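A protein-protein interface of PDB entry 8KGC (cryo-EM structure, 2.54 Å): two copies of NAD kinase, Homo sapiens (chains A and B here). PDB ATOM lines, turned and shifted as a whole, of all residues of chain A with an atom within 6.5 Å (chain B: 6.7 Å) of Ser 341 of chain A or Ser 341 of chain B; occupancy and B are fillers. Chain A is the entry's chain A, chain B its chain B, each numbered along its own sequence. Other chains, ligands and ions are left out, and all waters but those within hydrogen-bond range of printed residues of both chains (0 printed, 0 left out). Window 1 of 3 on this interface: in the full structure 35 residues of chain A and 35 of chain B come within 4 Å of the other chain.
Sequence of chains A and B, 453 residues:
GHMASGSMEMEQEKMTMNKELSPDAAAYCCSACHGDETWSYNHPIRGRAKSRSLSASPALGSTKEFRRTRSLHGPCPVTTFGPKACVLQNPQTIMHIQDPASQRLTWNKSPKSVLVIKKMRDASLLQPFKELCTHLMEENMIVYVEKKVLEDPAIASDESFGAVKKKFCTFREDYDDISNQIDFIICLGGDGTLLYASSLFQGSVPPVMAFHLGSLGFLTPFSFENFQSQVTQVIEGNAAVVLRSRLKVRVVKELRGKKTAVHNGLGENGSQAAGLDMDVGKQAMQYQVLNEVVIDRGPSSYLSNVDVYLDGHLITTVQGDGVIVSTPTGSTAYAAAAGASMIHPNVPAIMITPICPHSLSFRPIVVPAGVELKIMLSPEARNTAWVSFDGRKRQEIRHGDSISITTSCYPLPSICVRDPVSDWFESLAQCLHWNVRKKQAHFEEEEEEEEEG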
ATOM      1  N   SER A 331      19.120  32.039 -20.404  1.00  0.00           N
ATOM      2  CA  SER A 331      18.562  30.691 -20.416  1.00  0.00           C
ATOM      3  C   SER A 331      17.536  30.508 -19.307  1.00  0.00           C
ATOM      4  O   SER A 331      16.507  29.856 -19.507  1.00  0.00           O
ATOM      5  CB  SER A 331      19.682  29.662 -20.282  1.00  0.00           C
ATOM      6  OG  SER A 331      20.406  29.854 -19.081  1.00  0.00           O
ATOM      7  N   THR A 332      17.801  31.072 -18.130  1.00  0.00           N
ATOM      8  CA  THR A 332      16.869  31.019 -17.013  1.00  0.00           C
ATOM      9  C   THR A 332      15.818  32.117 -17.068  1.00  0.00           C
ATOM     10  O   THR A 332      14.913  32.135 -16.227  1.00  0.00           O
ATOM     11  CB  THR A 332      17.632  31.109 -15.691  1.00  0.00           C
ATOM     12  OG1 THR A 332      18.226  32.407 -15.574  1.00  0.00           O
ATOM     13  CG2 THR A 332      18.727  30.059 -15.649  1.00  0.00           C
ATOM     14  N   ALA A 335      13.228  32.662 -21.809  1.00  0.00           N
ATOM     15  CA  ALA A 335      13.520  31.472 -22.604  1.00  0.00           C
ATOM     16  C   ALA A 335      13.264  30.188 -21.826  1.00  0.00           C
ATOM     17  O   ALA A 335      12.868  29.177 -22.416  1.00  0.00           O
ATOM     18  CB  ALA A 335      14.965  31.511 -23.095  1.00  0.00           C
ATOM     19  N   ALA A 336      13.487  30.200 -20.510  1.00  0.00           N
ATOM     20  CA  ALA A 336      13.200  29.019 -19.703  1.00  0.00           C
ATOM     21  C   ALA A 336      11.715  28.688 -19.717  1.00  0.00           C
ATOM     22  O   ALA A 336      11.332  27.515 -19.756  1.00  0.00           O
ATOM     23  CB  ALA A 336      13.681  29.224 -18.268  1.00  0.00           C
ATOM     24  N   GLY A 339      10.443  26.366 -22.563  1.00  0.00           N
ATOM     25  CA  GLY A 339      10.897  24.997 -22.667  1.00  0.00           C
ATOM     26  C   GLY A 339      12.374  24.808 -22.923  1.00  0.00           C
ATOM     27  O   GLY A 339      12.794  23.678 -23.194  1.00  0.00           O
ATOM     28  N   ALA A 340      13.174  25.867 -22.848  1.00  0.00           N
ATOM     29  CA  ALA A 340      14.600  25.743 -23.091  1.00  0.00           C
ATOM     30  C   ALA A 340      15.284  25.028 -21.928  1.00  0.00           C
ATOM     31  O   ALA A 340      14.682  24.747 -20.889  1.00  0.00           O
ATOM     32  CB  ALA A 340      15.227  27.117 -23.312  1.00  0.00           C
ATOM     33  N   SER A 341      16.564  24.732 -22.118  1.00  0.00           N
ATOM     34  CA  SER A 341      17.370  24.045 -21.123  1.00  0.00           C
ATOM     35  C   SER A 341      18.229  25.042 -20.357  1.00  0.00           C
ATOM     36  O   SER A 341      18.692  26.043 -20.909  1.00  0.00           O
ATOM     37  CB  SER A 341      18.263  22.992 -21.779  1.00  0.00           C
ATOM     38  OG  SER A 341      17.493  22.077 -22.535  1.00  0.00           O
ATOM     39  N   MET A 342      18.438  24.758 -19.074  1.00  0.00           N
ATOM     40  CA  MET A 342      19.279  25.610 -18.245  1.00  0.00           C
ATOM     41  C   MET A 342      20.727  25.487 -18.699  1.00  0.00           C
ATOM     42  O   MET A 342      21.299  24.392 -18.677  1.00  0.00           O
ATOM     43  CB  MET A 342      19.147  25.217 -16.777  1.00  0.00           C
ATOM     44  CG  MET A 342      17.722  24.990 -16.300  1.00  0.00           C
ATOM     45  SD  MET A 342      16.711  26.479 -16.282  1.00  0.00           S
ATOM     46  CE  MET A 342      15.709  26.226 -17.741  1.00  0.00           C
ATOM     47  N   ILE A 343      21.323  26.603 -19.107  1.00  0.00           N
ATOM     48  CA  ILE A 343      22.691  26.632 -19.608  1.00  0.00           C
ATOM     49  C   ILE A 343      23.534  27.485 -18.673  1.00  0.00           C
ATOM     50  O   ILE A 343      23.164  28.620 -18.355  1.00  0.00           O
ATOM     51  CB  ILE A 343      22.755  27.168 -21.047  1.00  0.00           C
ATOM     52  CG1 ILE A 343      22.021  26.221 -21.996  1.00  0.00           C
ATOM     53  CG2 ILE A 343      24.197  27.346 -21.484  1.00  0.00           C
ATOM     54  CD1 ILE A 343      22.273  26.504 -23.453  1.00  0.00           C
ATOM     55  N   MET A 351      21.093  30.468 -27.909  1.00  0.00           N
ATOM     56  CA  MET A 351      19.936  29.588 -27.854  1.00  0.00           C
ATOM     57  C   MET A 351      18.813  30.150 -28.712  1.00  0.00           C
ATOM     58  O   MET A 351      18.529  31.350 -28.661  1.00  0.00           O
ATOM     59  CB  MET A 351      19.454  29.419 -26.416  1.00  0.00           C
ATOM     60  CG  MET A 351      20.566  29.208 -25.417  1.00  0.00           C
ATOM     61  SD  MET A 351      19.915  29.133 -23.745  1.00  0.00           S
ATOM     62  CE  MET A 351      18.763  27.775 -23.909  1.00  0.00           C
ATOM     63  N   THR A 353      14.801  29.451 -29.228  1.00  0.00           N
ATOM     64  CA  THR A 353      13.698  28.764 -28.577  1.00  0.00           C
ATOM     65  C   THR A 353      12.374  29.268 -29.142  1.00  0.00           C
ATOM     66  O   THR A 353      12.117  30.479 -29.124  1.00  0.00           O
ATOM     67  CB  THR A 353      13.742  28.979 -27.063  1.00  0.00           C
ATOM     68  OG1 THR A 353      15.054  28.675 -26.575  1.00  0.00           O
ATOM     69  CG2 THR A 353      12.737  28.080 -26.375  1.00  0.00           C
ATOM     70  N   ARG A 363      12.015  21.469 -31.288  1.00  0.00           N
ATOM     71  CA  ARG A 363      12.760  21.481 -30.040  1.00  0.00           C
ATOM     72  C   ARG A 363      13.754  22.642 -30.040  1.00  0.00           C
ATOM     73  O   ARG A 363      14.345  22.949 -31.078  1.00  0.00           O
ATOM     74  CB  ARG A 363      13.493  20.155 -29.851  1.00  0.00           C
ATOM     75  CG  ARG A 363      14.055  19.935 -28.464  1.00  0.00           C
ATOM     76  CD  ARG A 363      14.019  18.471 -28.087  1.00  0.00           C
ATOM     77  NE  ARG A 363      12.658  17.957 -28.038  1.00  0.00           N
ATOM     78  CZ  ARG A 363      12.340  16.721 -27.680  1.00  0.00           C
ATOM     79  NH1 ARG A 363      13.266  15.845 -27.328  1.00  0.00           N
ATOM     80  NH2 ARG A 363      11.062  16.355 -27.677  1.00  0.00           N
ATOM     81  N   PRO A 364      13.945  23.313 -28.903  1.00  0.00           N
ATOM     82  CA  PRO A 364      14.900  24.426 -28.857  1.00  0.00           C
ATOM     83  C   PRO A 364      16.300  23.969 -29.232  1.00  0.00           C
ATOM     84  O   PRO A 364      16.714  22.852 -28.924  1.00  0.00           O
ATOM     85  CB  PRO A 364      14.837  24.886 -27.398  1.00  0.00           C
ATOM     86  CG  PRO A 364      13.495  24.464 -26.932  1.00  0.00           C
ATOM     87  CD  PRO A 364      13.188  23.185 -27.646  1.00  0.00           C
ATOM     88  N   ILE A 365      17.033  24.849 -29.911  1.00  0.00           N
ATOM     89  CA  ILE A 365      18.353  24.498 -30.410  1.00  0.00           C
ATOM     90  C   ILE A 365      19.392  25.439 -29.816  1.00  0.00           C
ATOM     91  O   ILE A 365      19.084  26.526 -29.323  1.00  0.00           O
ATOM     92  CB  ILE A 365      18.429  24.519 -31.951  1.00  0.00           C
ATOM     93  CG1 ILE A 365      18.365  25.951 -32.474  1.00  0.00           C
ATOM     94  CG2 ILE A 365      17.315  23.685 -32.548  1.00  0.00           C
ATOM     95  CD1 ILE A 365      18.518  26.052 -33.971  1.00  0.00           C
ATOM     96  N   VAL A 366      20.644  24.994 -29.869  1.00  0.00           N
ATOM     97  CA  VAL A 366      21.787  25.743 -29.369  1.00  0.00           C
ATOM     98  C   VAL A 366      22.841  25.774 -30.466  1.00  0.00           C
ATOM     99  O   VAL A 366      23.206  24.725 -31.008  1.00  0.00           O
ATOM    100  CB  VAL A 366      22.356  25.117 -28.083  1.00  0.00           C
ATOM    101  CG1 VAL A 366      23.614  25.831 -27.663  1.00  0.00           C
ATOM    102  CG2 VAL A 366      21.323  25.161 -26.973  1.00  0.00           C
ATOM    103  N   SER B 331      23.813  14.947 -28.410  1.00  0.00           N
ATOM    104  CA  SER B 331      22.583  15.687 -28.152  1.00  0.00           C
ATOM    105  C   SER B 331      21.432  15.154 -28.992  1.00  0.00           C
ATOM    106  O   SER B 331      20.301  15.046 -28.508  1.00  0.00           O
ATOM    107  CB  SER B 331      22.798  17.173 -28.428  1.00  0.00           C
ATOM    108  OG  SER B 331      23.186  17.387 -29.772  1.00  0.00           O
ATOM    109  N   THR B 332      21.700  14.823 -30.253  1.00  0.00           N
ATOM    110  CA  THR B 332      20.690  14.243 -31.129  1.00  0.00           C
ATOM    111  C   THR B 332      20.551  12.739 -30.950  1.00  0.00           C
ATOM    112  O   THR B 332      19.665  12.134 -31.564  1.00  0.00           O
ATOM    113  CB  THR B 332      21.025  14.558 -32.585  1.00  0.00           C
ATOM    114  OG1 THR B 332      22.192  13.824 -32.974  1.00  0.00           O
ATOM    115  CG2 THR B 332      21.304  16.041 -32.742  1.00  0.00           C
ATOM    116  N   ALA B 335      20.009  11.003 -25.872  1.00  0.00           N
ATOM    117  CA  ALA B 335      19.739  12.162 -25.026  1.00  0.00           C
ATOM    118  C   ALA B 335      18.574  12.985 -25.562  1.00  0.00           C
ATOM    119  O   ALA B 335      17.805  13.562 -24.785  1.00  0.00           O
ATOM    120  CB  ALA B 335      20.992  13.027 -24.903  1.00  0.00           C
ATOM    121  N   ALA B 336      18.434  13.065 -26.888  1.00  0.00           N
ATOM    122  CA  ALA B 336      17.311  13.797 -27.469  1.00  0.00           C
ATOM    123  C   ALA B 336      15.980  13.162 -27.104  1.00  0.00           C
ATOM    124  O   ALA B 336      14.985  13.870 -26.917  1.00  0.00           O
ATOM    125  CB  ALA B 336      17.452  13.874 -28.987  1.00  0.00           C
ATOM    126  N   GLY B 339      14.335  14.543 -23.925  1.00  0.00           N
ATOM    127  CA  GLY B 339      13.927  15.929 -23.862  1.00  0.00           C
ATOM    128  C   GLY B 339      15.039  16.950 -23.928  1.00  0.00           C
ATOM    129  O   GLY B 339      14.768  18.143 -23.755  1.00  0.00           O
ATOM    130  N   ALA B 340      16.276  16.529 -24.170  1.00  0.00           N
ATOM    131  CA  ALA B 340      17.382  17.468 -24.247  1.00  0.00           C
ATOM    132  C   ALA B 340      17.281  18.320 -25.507  1.00  0.00           C
ATOM    133  O   ALA B 340      16.668  17.935 -26.504  1.00  0.00           O
ATOM    134  CB  ALA B 340      18.716  16.726 -24.222  1.00  0.00           C
ATOM    135  N   SER B 341      17.895  19.497 -25.450  1.00  0.00           N
ATOM    136  CA  SER B 341      17.888  20.414 -26.580  1.00  0.00           C
ATOM    137  C   SER B 341      18.976  20.042 -27.576  1.00  0.00           C
ATOM    138  O   SER B 341      20.078  19.642 -27.191  1.00  0.00           O
ATOM    139  CB  SER B 341      18.089  21.850 -26.100  1.00  0.00           C
ATOM    140  OG  SER B 341      17.105  22.207 -25.150  1.00  0.00           O
ATOM    141  N   MET B 342      18.664  20.177 -28.860  1.00  0.00           N
ATOM    142  CA  MET B 342      19.642  19.886 -29.899  1.00  0.00           C
ATOM    143  C   MET B 342      20.754  20.925 -29.863  1.00  0.00           C
ATOM    144  O   MET B 342      20.494  22.128 -29.944  1.00  0.00           O
ATOM    145  CB  MET B 342      18.972  19.875 -31.270  1.00  0.00           C
ATOM    146  CG  MET B 342      17.492  19.540 -31.233  1.00  0.00           C
ATOM    147  SD  MET B 342      17.144  17.925 -30.518  1.00  0.00           S
ATOM    148  CE  MET B 342      17.831  16.850 -31.770  1.00  0.00           C
ATOM    149  N   ILE B 343      21.994  20.461 -29.745  1.00  0.00           N
ATOM    150  CA  ILE B 343      23.155  21.335 -29.621  1.00  0.00           C
ATOM    151  C   ILE B 343      24.084  21.081 -30.799  1.00  0.00           C
ATOM    152  O   ILE B 343      24.404  19.928 -31.106  1.00  0.00           O
ATOM    153  CB  ILE B 343      23.890  21.119 -28.287  1.00  0.00           C
ATOM    154  CG1 ILE B 343      22.994  21.531 -27.120  1.00  0.00           C
ATOM    155  CG2 ILE B 343      25.187  21.903 -28.262  1.00  0.00           C
ATOM    156  CD1 ILE B 343      23.720  21.622 -25.801  1.00  0.00           C
ATOM    157  N   HIS B 344      24.505  22.154 -31.453  1.00  0.00           N
ATOM    158  CA  HIS B 344      25.444  22.041 -32.559  1.00  0.00           C
ATOM    159  C   HIS B 344      26.772  21.492 -32.049  1.00  0.00           C
ATOM    160  O   HIS B 344      27.229  21.894 -30.974  1.00  0.00           O
ATOM    161  CB  HIS B 344      25.645  23.405 -33.213  1.00  0.00           C
ATOM    162  CG  HIS B 344      26.396  23.354 -34.505  1.00  0.00           C
ATOM    163  ND1 HIS B 344      27.768  23.244 -34.566  1.00  0.00           N
ATOM    164  CD2 HIS B 344      25.967  23.406 -35.788  1.00  0.00           C
ATOM    165  CE1 HIS B 344      28.151  23.225 -35.828  1.00  0.00           C
ATOM    166  NE2 HIS B 344      27.078  23.323 -36.591  1.00  0.00           N
ATOM    167  N   MET B 351      26.172  17.979 -21.563  1.00  0.00           N
ATOM    168  CA  MET B 351      24.748  17.979 -21.274  1.00  0.00           C
ATOM    169  C   MET B 351      24.418  16.929 -20.226  1.00  0.00           C
ATOM    170  O   MET B 351      24.909  15.799 -20.289  1.00  0.00           O
ATOM    171  CB  MET B 351      23.940  17.708 -22.541  1.00  0.00           C
ATOM    172  CG  MET B 351      24.399  18.500 -23.740  1.00  0.00           C
ATOM    173  SD  MET B 351      23.343  18.166 -25.150  1.00  0.00           S
ATOM    174  CE  MET B 351      21.758  18.664 -24.487  1.00  0.00           C
ATOM    175  N   THR B 353      21.050  15.131 -18.757  1.00  0.00           N
ATOM    176  CA  THR B 353      19.639  14.972 -19.069  1.00  0.00           C
ATOM    177  C   THR B 353      19.053  13.841 -18.232  1.00  0.00           C
ATOM    178  O   THR B 353      19.578  12.718 -18.257  1.00  0.00           O
ATOM    179  CB  THR B 353      19.439  14.687 -20.559  1.00  0.00           C
ATOM    180  OG1 THR B 353      20.183  15.637 -21.329  1.00  0.00           O
ATOM    181  CG2 THR B 353      17.973  14.797 -20.921  1.00  0.00           C
ATOM    182  N   ARG B 363      14.892  20.000 -15.277  1.00  0.00           N
ATOM    183  CA  ARG B 363      15.150  20.446 -16.633  1.00  0.00           C
ATOM    184  C   ARG B 363      16.585  20.112 -17.022  1.00  0.00           C
ATOM    185  O   ARG B 363      17.486  20.220 -16.184  1.00  0.00           O
ATOM    186  CB  ARG B 363      14.921  21.959 -16.752  1.00  0.00           C
ATOM    187  CG  ARG B 363      14.825  22.485 -18.171  1.00  0.00           C
ATOM    188  CD  ARG B 363      13.563  22.002 -18.861  1.00  0.00           C
ATOM    189  NE  ARG B 363      12.357  22.570 -18.271  1.00  0.00           N
ATOM    190  CZ  ARG B 363      11.800  23.708 -18.663  1.00  0.00           C
ATOM    191  NH1 ARG B 363      12.328  24.439 -19.628  1.00  0.00           N
ATOM    192  NH2 ARG B 363      10.684  24.120 -18.069  1.00  0.00           N
ATOM    193  N   PRO B 364      16.829  19.689 -18.262  1.00  0.00           N
ATOM    194  CA  PRO B 364      18.196  19.333 -18.661  1.00  0.00           C
ATOM    195  C   PRO B 364      19.162  20.496 -18.486  1.00  0.00           C
ATOM    196  O   PRO B 364      18.816  21.656 -18.709  1.00  0.00           O
ATOM    197  CB  PRO B 364      18.042  18.948 -20.134  1.00  0.00           C
ATOM    198  CG  PRO B 364      16.642  18.471 -20.240  1.00  0.00           C
ATOM    199  CD  PRO B 364      15.844  19.311 -19.289  1.00  0.00           C
ATOM    200  N   ILE B 365      20.384  20.169 -18.079  1.00  0.00           N
ATOM    201  CA  ILE B 365      21.418  21.155 -17.803  1.00  0.00           C
ATOM    202  C   ILE B 365      22.454  21.111 -18.913  1.00  0.00           C
ATOM    203  O   ILE B 365      22.700  20.067 -19.527  1.00  0.00           O
ATOM    204  CB  ILE B 365      22.105  20.912 -16.445  1.00  0.00           C
ATOM    205  CG1 ILE B 365      21.152  20.249 -15.458  1.00  0.00           C
ATOM    206  CG2 ILE B 365      22.630  22.209 -15.873  1.00  0.00           C
ATOM    207  CD1 ILE B 365      21.871  19.663 -14.271  1.00  0.00           C
ATOM    208  N   VAL B 366      23.083  22.257 -19.153  1.00  0.00           N
ATOM    209  CA  VAL B 366      24.239  22.364 -20.032  1.00  0.00           C
ATOM    210  C   VAL B 366      25.337  23.061 -19.244  1.00  0.00           C
ATOM    211  O   VAL B 366      25.154  24.196 -18.793  1.00  0.00           O
ATOM    212  CB  VAL B 366      23.915  23.132 -21.322  1.00  0.00           C
ATOM    213  CG1 VAL B 366      25.161  23.312 -22.153  1.00  0.00           C
ATOM    214  CG2 VAL B 366      22.848  22.401 -22.114  1.00  0.00           C
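O of Met 342 of chain B sits at hydrogen-bond distance from N of Val 366 of chain A, at 2.9 Å.
The backbone carbonyl oxygen (O) of Ala 336 of chain A sits at hydrogen-bond distance from the guanidinium group (NH1) of Arg 363 of chain B (3.2 Å).
The side-chain hydroxyl (OG) of Ser 341 of chain A lies within hydrogen-bond range of the side-chain hydroxyl (OG) of Ser 341 of chain B, 2.6 Å away.
O of Ala 336 of chain B sits at hydrogen-bond distance from NH1 of Arg 363 of chain A (2.7 Å).
O of Val 366 of chain A sits at hydrogen-bond distance from N of His 344 of chain B (2.9 Å).
The backbone carbonyl oxygen of Pro 364 of chain B is in hydrogen-bond range of the backbone NH of Met 342 of chain A, 3.1 Å away.
O of Ala 340 of chain A is in hydrogen-bond range of NH1 of Arg 363 of chain B (2.7 Å).
N of Met 342 of chain B is in hydrogen-bond range of O of Pro 364 of chain A.
N of Val 366 of chain B lies within hydrogen-bond range of O of Met 342 of chain A (2.8 Å).
O of Ser 331 of chain B sits close to N of Ala 336 of chain B, at 3.2 Å.
The backbone carbonyl oxygen (O) of Ala 335 of chain B sits close to the backbone NH (N) of Ala 340 of chain B (3.4 Å).
O of Ser 331 of chain A sits close to N of Ala 336 of chain A (3.2 Å).
The backbone carbonyl oxygen (O) of Ile 343 of chain B lies within hydrogen-bond range of the side-chain hydroxyl (OG) of Ser 331 of chain B, at 3.1 Å.
The side-chain hydroxyl (OG) of Ser 331 of chain A lies within hydrogen-bond range of the backbone carbonyl oxygen (O) of Ile 343 of chain A, at 3.1 Å.
N of Ala 340 of chain A lies close to O of Ala 335 of chain A (3.4 Å).
C of Gly 339 of chain A touches NH1 of Arg 363 of chain B, at 3.3 Å.
CB of Ser 341 of chain A touches O of Pro 364 of chain B, at 3.4 Å.
Met 342 of chain A touches Arg 363 of chain B.
Met 342 of chain A touches Ile 365 of chain B.
Ile 343 of chain A touches Val 366 of chain B (CA to O, 3.6 Å).
NH1 of Arg 363 of chain A touches CA of Gly 339 of chain B, at 3.5 Å.
Arg 363 of chain A touches Ala 340 of chain B.
CD of Arg 363 of chain A touches SD of Met 342 of chain B, at 3.997 Å.
Ile 365 of chain A touches Met 342 of chain B.
Ile 343 of chain B touches Val 366 of chain A.
Ser 341 of chain A touches two residues of chain B.
Ser 341 of chain B touches just these residues of chain A: Ser 341 and Pro 364.
Printed residues of chain A within 4 Å of Val 366 of chain B: Met 342 (2.8 Å) and Ile 343 (3.6 Å).
Printed residues of chain A within 4 Å of Met 342 of chain B: Arg 363, Pro 364, Ile 365 and Val 366.
Of the printed residues of chain B, Ala 340 of chain A touches Arg 363 (2.7 Å).
Of the printed residues of chain A, Ile 365 of chain B touches Met 342.
Printed residues of chain B within 4 Å of Ala 336 of chain A: Arg 363.
Ser 331 of chain A touches none of the printed residues of chain B.
Ser 331 of chain B touches none of the printed residues of chain A.
The nearest residue of chain B that does not touch Ser 341 of chain A is Arg 363 of chain B (4.2 Å).
Along chain A the printed residues that touch a printed residue of chain B span positions 336 to 366.
Along chain B the printed residues that touch a printed residue of chain A span positions 336 to 366.
Among the printed residues, 20 pairs touch across the chains.
Ala 336 of chain A touches Arg 363 of chain B, and with the chains exchanged Arg 363 of chain A touches Ala 336 of chain B.
Gly 339 of chain A touches Arg 363 of chain B, and with the chains exchanged Arg 363 of chain A touches Gly 339 of chain B.
Ser 341 of chain A touches its own counterpart, Ser 341 of chain B.
Ile 343 of chain A touches Val 366 of chain B, and with the chains exchanged Val 366 of chain A touches Ile 343 of chain B.
Positions printed for both chains: 331, 332, 335, 336, 339, 340, 341, 342, 343, 351, 353, 363, 364, 365 and 366.
Of the 20 pairs that touch across the chains among the printed residues, 19 have their exchanged pair printed and touching as well.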
